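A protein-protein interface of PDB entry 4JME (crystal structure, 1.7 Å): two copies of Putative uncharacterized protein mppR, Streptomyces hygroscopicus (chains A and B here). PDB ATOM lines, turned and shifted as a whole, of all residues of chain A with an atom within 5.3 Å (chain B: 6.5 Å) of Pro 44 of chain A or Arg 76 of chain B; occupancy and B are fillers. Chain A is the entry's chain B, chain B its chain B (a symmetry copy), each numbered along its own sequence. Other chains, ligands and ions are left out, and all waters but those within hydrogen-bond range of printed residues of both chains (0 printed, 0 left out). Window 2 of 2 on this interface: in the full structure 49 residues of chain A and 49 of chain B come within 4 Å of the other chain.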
ATOM      1  N   GLY A  34      33.714  -8.860  22.688  1.00  0.00           N
ATOM      2  CA  GLY A  34      32.374  -8.378  22.385  1.00  0.00           C
ATOM      3  C   GLY A  34      32.384  -7.531  21.136  1.00  0.00           C
ATOM      4  O   GLY A  34      33.429  -7.337  20.496  1.00  0.00           O
ATOM      5  N   PRO A  35      31.213  -7.022  20.764  1.00  0.00           N
ATOM      6  CA  PRO A  35      31.168  -6.033  19.686  1.00  0.00           C
ATOM      7  C   PRO A  35      31.866  -4.732  20.086  1.00  0.00           C
ATOM      8  O   PRO A  35      31.994  -4.433  21.279  1.00  0.00           O
ATOM      9  CB  PRO A  35      29.655  -5.839  19.475  1.00  0.00           C
ATOM     10  CG  PRO A  35      29.057  -6.151  20.772  1.00  0.00           C
ATOM     11  CD  PRO A  35      29.889  -7.238  21.372  1.00  0.00           C
ATOM     12  N   VAL A  36      32.294  -3.962  19.089  1.00  0.00           N
ATOM     13  CA  VAL A  36      33.107  -2.776  19.313  1.00  0.00           C
ATOM     14  C   VAL A  36      32.585  -1.532  18.612  1.00  0.00           C
ATOM     15  O   VAL A  36      31.603  -1.567  17.866  1.00  0.00           O
ATOM     16  CB  VAL A  36      34.570  -3.043  18.830  1.00  0.00           C
ATOM     17  CG1 VAL A  36      35.104  -4.285  19.503  1.00  0.00           C
ATOM     18  CG2 VAL A  36      34.632  -3.206  17.311  1.00  0.00           C
ATOM     19  N   LEU A  42      27.356  -0.699  19.139  1.00  0.00           N
ATOM     20  CA  LEU A  42      28.521  -1.573  18.976  1.00  0.00           C
ATOM     21  C   LEU A  42      28.185  -2.570  17.886  1.00  0.00           C
ATOM     22  O   LEU A  42      27.006  -2.894  17.661  1.00  0.00           O
ATOM     23  CB  LEU A  42      28.846  -2.307  20.271  1.00  0.00           C
ATOM     24  CG  LEU A  42      29.029  -1.423  21.504  1.00  0.00           C
ATOM     25  CD1 LEU A  42      29.245  -2.337  22.710  1.00  0.00           C
ATOM     26  CD2 LEU A  42      30.163  -0.465  21.359  1.00  0.00           C
ATOM     27  N   SER A  43      29.208  -3.020  17.182  1.00  0.00           N
ATOM     28  CA  SER A  43      29.028  -4.004  16.128  1.00  0.00           C
ATOM     29  C   SER A  43      30.289  -4.813  15.952  1.00  0.00           C
ATOM     30  O   SER A  43      31.361  -4.434  16.416  1.00  0.00           O
ATOM     31  CB  SER A  43      28.653  -3.311  14.807  1.00  0.00           C
ATOM     32  OG  SER A  43      29.632  -2.369  14.410  1.00  0.00           O
ATOM     33  N   PRO A  44      30.164  -5.973  15.310  1.00  0.00           N
ATOM     34  CA  PRO A  44      31.364  -6.803  15.157  1.00  0.00           C
ATOM     35  C   PRO A  44      32.568  -6.106  14.478  1.00  0.00           C
ATOM     36  O   PRO A  44      33.699  -6.340  14.934  1.00  0.00           O
ATOM     37  CB  PRO A  44      30.849  -7.978  14.332  1.00  0.00           C
ATOM     38  CG  PRO A  44      29.402  -8.070  14.717  1.00  0.00           C
ATOM     39  CD  PRO A  44      28.957  -6.647  14.815  1.00  0.00           C
ATOM     40  N   THR A  45      32.353  -5.282  13.447  1.00  0.00           N
ATOM     41  CA  THR A  45      33.445  -4.582  12.766  1.00  0.00           C
ATOM     42  C   THR A  45      33.720  -3.180  13.295  1.00  0.00           C
ATOM     43  O   THR A  45      34.761  -2.606  12.993  1.00  0.00           O
ATOM     44  CB  THR A  45      33.174  -4.410  11.249  1.00  0.00           C
ATOM     45  OG1 THR A  45      32.136  -3.452  11.040  1.00  0.00           O
ATOM     46  CG2 THR A  45      32.778  -5.723  10.610  1.00  0.00           C
ATOM     47  N   GLY A  46      32.786  -2.619  14.055  1.00  0.00           N
ATOM     48  CA  GLY A  46      32.900  -1.238  14.484  1.00  0.00           C
ATOM     49  C   GLY A  46      32.298  -0.237  13.515  1.00  0.00           C
ATOM     50  O   GLY A  46      32.284   0.970  13.783  1.00  0.00           O
ATOM     51  N   PRO B  71      21.979 -17.520  14.113  1.00  0.00           N
ATOM     52  CA  PRO B  71      22.389 -17.463  15.525  1.00  0.00           C
ATOM     53  C   PRO B  71      23.856 -17.101  15.703  1.00  0.00           C
ATOM     54  O   PRO B  71      24.240 -16.519  16.717  1.00  0.00           O
ATOM     55  CB  PRO B  71      22.158 -18.894  16.035  1.00  0.00           C
ATOM     56  CG  PRO B  71      21.533 -19.650  14.936  1.00  0.00           C
ATOM     57  CD  PRO B  71      21.707 -18.896  13.667  1.00  0.00           C
ATOM     58  N   ASP B  72      24.683 -17.472  14.736  1.00  0.00           N
ATOM     59  CA  ASP B  72      26.099 -17.159  14.835  1.00  0.00           C
ATOM     60  C   ASP B  72      26.324 -15.663  14.624  1.00  0.00           C
ATOM     61  O   ASP B  72      27.216 -15.075  15.237  1.00  0.00           O
ATOM     62  CB  ASP B  72      26.903 -17.982  13.822  1.00  0.00           C
ATOM     63  CG  ASP B  72      26.776 -19.496  14.049  1.00  0.00           C
ATOM     64  OD1 ASP B  72      26.648 -19.947  15.211  1.00  0.00           O
ATOM     65  OD2 ASP B  72      26.798 -20.238  13.054  1.00  0.00           O
ATOM     66  N   ALA B  73      25.506 -15.059  13.767  1.00  0.00           N
ATOM     67  CA  ALA B  73      25.551 -13.612  13.544  1.00  0.00           C
ATOM     68  C   ALA B  73      25.107 -12.880  14.798  1.00  0.00           C
ATOM     69  O   ALA B  73      25.748 -11.908  15.223  1.00  0.00           O
ATOM     70  CB  ALA B  73      24.677 -13.215  12.370  1.00  0.00           C
ATOM     71  N   ALA B  74      24.001 -13.331  15.379  1.00  0.00           N
ATOM     72  CA  ALA B  74      23.474 -12.731  16.606  1.00  0.00           C
ATOM     73  C   ALA B  74      24.496 -12.790  17.740  1.00  0.00           C
ATOM     74  O   ALA B  74      24.671 -11.831  18.488  1.00  0.00           O
ATOM     75  CB  ALA B  74      22.173 -13.407  17.017  1.00  0.00           C
ATOM     76  N   ARG B  75      25.174 -13.922  17.864  1.00  0.00           N
ATOM     77  CA  ARG B  75      26.175 -14.107  18.904  1.00  0.00           C
ATOM     78  C   ARG B  75      27.248 -13.014  18.920  1.00  0.00           C
ATOM     79  O   ARG B  75      27.731 -12.623  19.973  1.00  0.00           O
ATOM     80  CB  ARG B  75      26.846 -15.460  18.712  1.00  0.00           C
ATOM     81  CG  ARG B  75      27.891 -15.758  19.729  1.00  0.00           C
ATOM     82  CD  ARG B  75      28.288 -17.217  19.612  1.00  0.00           C
ATOM     83  NE  ARG B  75      28.539 -17.818  20.916  1.00  0.00           N
ATOM     84  CZ  ARG B  75      28.464 -19.122  21.158  1.00  0.00           C
ATOM     85  NH1 ARG B  75      28.134 -19.966  20.186  1.00  0.00           N
ATOM     86  NH2 ARG B  75      28.709 -19.582  22.380  1.00  0.00           N
ATOM     87  N   ARG B  76      27.621 -12.521  17.750  1.00  0.00           N
ATOM     88  CA  ARG B  76      28.703 -11.551  17.671  1.00  0.00           C
ATOM     89  C   ARG B  76      28.316 -10.174  18.203  1.00  0.00           C
ATOM     90  O   ARG B  76      29.190  -9.330  18.450  1.00  0.00           O
ATOM     91  CB  ARG B  76      29.200 -11.454  16.236  1.00  0.00           C
ATOM     92  CG  ARG B  76      29.766 -12.789  15.765  1.00  0.00           C
ATOM     93  CD  ARG B  76      30.288 -12.681  14.372  1.00  0.00           C
ATOM     94  NE  ARG B  76      31.520 -11.898  14.316  1.00  0.00           N
ATOM     95  CZ  ARG B  76      31.980 -11.336  13.204  1.00  0.00           C
ATOM     96  NH1 ARG B  76      31.304 -11.457  12.066  1.00  0.00           N
ATOM     97  NH2 ARG B  76      33.097 -10.634  13.226  1.00  0.00           N
ATOM     98  N   PHE B  77      27.016  -9.960  18.395  1.00  0.00           N
ATOM     99  CA  PHE B  77      26.515  -8.716  18.971  1.00  0.00           C
ATOM    100  C   PHE B  77      26.353  -8.835  20.492  1.00  0.00           C
ATOM    101  O   PHE B  77      26.019  -7.857  21.160  1.00  0.00           O
ATOM    102  CB  PHE B  77      25.163  -8.361  18.350  1.00  0.00           C
ATOM    103  CG  PHE B  77      25.268  -7.733  17.003  1.00  0.00           C
ATOM    104  CD1 PHE B  77      25.392  -6.364  16.892  1.00  0.00           C
ATOM    105  CD2 PHE B  77      25.270  -8.501  15.845  1.00  0.00           C
ATOM    106  CE1 PHE B  77      25.498  -5.746  15.648  1.00  0.00           C
ATOM    107  CE2 PHE B  77      25.384  -7.891  14.608  1.00  0.00           C
ATOM    108  CZ  PHE B  77      25.490  -6.516  14.503  1.00  0.00           C
ATOM    109  N   LEU B  78      26.576 -10.021  21.042  1.00  0.00           N
ATOM    110  CA  LEU B  78      26.476 -10.207  22.487  1.00  0.00           C
ATOM    111  C   LEU B  78      27.827  -9.974  23.155  1.00  0.00           C
ATOM    112  O   LEU B  78      28.800 -10.696  22.894  1.00  0.00           O
ATOM    113  CB  LEU B  78      25.961 -11.612  22.830  1.00  0.00           C
ATOM    114  CG  LEU B  78      24.667 -12.039  22.138  1.00  0.00           C
ATOM    115  CD1 LEU B  78      24.359 -13.489  22.484  1.00  0.00           C
ATOM    116  CD2 LEU B  78      23.514 -11.142  22.511  1.00  0.00           C
ATOM    117  N   PRO B  79      27.905  -8.955  24.018  1.00  0.00           N
ATOM    118  CA  PRO B  79      29.150  -8.693  24.756  1.00  0.00           C
ATOM    119  C   PRO B  79      29.432  -9.786  25.785  1.00  0.00           C
ATOM    120  O   PRO B  79      28.537 -10.541  26.136  1.00  0.00           O
ATOM    121  CB  PRO B  79      28.870  -7.366  25.460  1.00  0.00           C
ATOM    122  CG  PRO B  79      27.380  -7.301  25.596  1.00  0.00           C
ATOM    123  CD  PRO B  79      26.795  -8.086  24.455  1.00  0.00           C
ATOM    124  N   TYR B 137      20.324  -2.631  17.872  1.00  0.00           N
ATOM    125  CA  TYR B 137      20.018  -1.463  17.034  1.00  0.00           C
ATOM    126  C   TYR B 137      18.665  -0.873  17.445  1.00  0.00           C
ATOM    127  O   TYR B 137      17.710  -1.610  17.659  1.00  0.00           O
ATOM    128  CB  TYR B 137      19.968  -1.807  15.545  1.00  0.00           C
ATOM    129  CG  TYR B 137      21.286  -2.206  14.945  1.00  0.00           C
ATOM    130  CD1 TYR B 137      22.209  -1.260  14.543  1.00  0.00           C
ATOM    131  CD2 TYR B 137      21.612  -3.549  14.807  1.00  0.00           C
ATOM    132  CE1 TYR B 137      23.433  -1.637  14.003  1.00  0.00           C
ATOM    133  CE2 TYR B 137      22.823  -3.927  14.271  1.00  0.00           C
ATOM    134  CZ  TYR B 137      23.725  -2.970  13.873  1.00  0.00           C
ATOM    135  OH  TYR B 137      24.941  -3.371  13.337  1.00  0.00           O
ATOM    136  N   ASP B 264      27.198  -4.971   8.754  1.00  0.00           N
ATOM    137  CA  ASP B 264      27.070  -5.469  10.127  1.00  0.00           C
ATOM    138  C   ASP B 264      25.576  -5.634  10.466  1.00  0.00           C
ATOM    139  O   ASP B 264      25.154  -6.666  10.985  1.00  0.00           O
ATOM    140  CB  ASP B 264      27.790  -4.544  11.122  1.00  0.00           C
ATOM    141  CG  ASP B 264      29.295  -4.812  11.195  1.00  0.00           C
ATOM    142  OD1 ASP B 264      29.863  -5.304  10.201  1.00  0.00           O
ATOM    143  OD2 ASP B 264      29.921  -4.541  12.240  1.00  0.00           O
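OD2 of Asp 264 of chain B sits at hydrogen-bond distance from OG of Ser 43 of chain A (3.1 Å). OD2 of Asp 264 of chain B lies within hydrogen-bond range of OG1 of Thr 45 of chain A (2.7 Å). The backbone nitrogen of Pro 44 of chain A lies close to the side-chain carboxylate of Asp 264 of chain B (3.4 Å).
The backbone NH (N) of Val 36 of chain A is in hydrogen-bond range of the backbone carbonyl oxygen (O) of Ser 43 of chain A. OG of Ser 43 of chain A sits at hydrogen-bond distance from N of Gly 46 of chain A, at 3.2 Å.
Pro 35 of chain A touches Arg 76 of chain B. Phe 77 of chain B touches Pro 35 of chain A. Leu 78 of chain B touches Pro 35 of chain A. N of Pro 79 of chain B touches CD of Pro 35 of chain A (3.7 Å). Leu 42 of chain A touches Phe 77 of chain B. CE1 of Phe 77 of chain B touches CA of Ser 43 of chain A, 3.97 Å away. CB of Ser 43 of chain A touches OH of Tyr 137 of chain B, 3.99 Å away. Pro 44 of chain A touches Arg 76 of chain B. Pro 44 of chain A touches Phe 77 of chain B (CD to CZ, 3.5 Å). Gly 46 of chain A touches Asp 264 of chain B (N to OD2, 3.9 Å).
Pro 44 of chain A touches just these residues of chain B: Arg 76, Phe 77 and Asp 264. Arg 76 of chain B touches two residues of chain A. Of the printed residues of chain A, Leu 78 of chain B touches Pro 35 (3.9 Å). Printed residues of chain A within 4 Å of Pro 79 of chain B: Pro 35. Arg 75 of chain B touches none of the printed residues of chain A. The nearest residue of chain A that does not touch Arg 76 of chain B is Gly 34 of chain A (4.5 Å). The nearest printed residue of chain B that does not touch Ser 43 of chain A is Arg 76 of chain B (5.3 Å).
Of the 8 printed residues of chain A, 6 touch a printed residue of chain B. Hydrophobic or aromatic side chains of chain A that line the printed part of chain B: Pro 35 and Pro 44. Hydrophobic or aromatic side chains of chain B within 4 Å of the printed part of chain A: Phe 77 and Tyr 137.
No position is printed for both chains.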
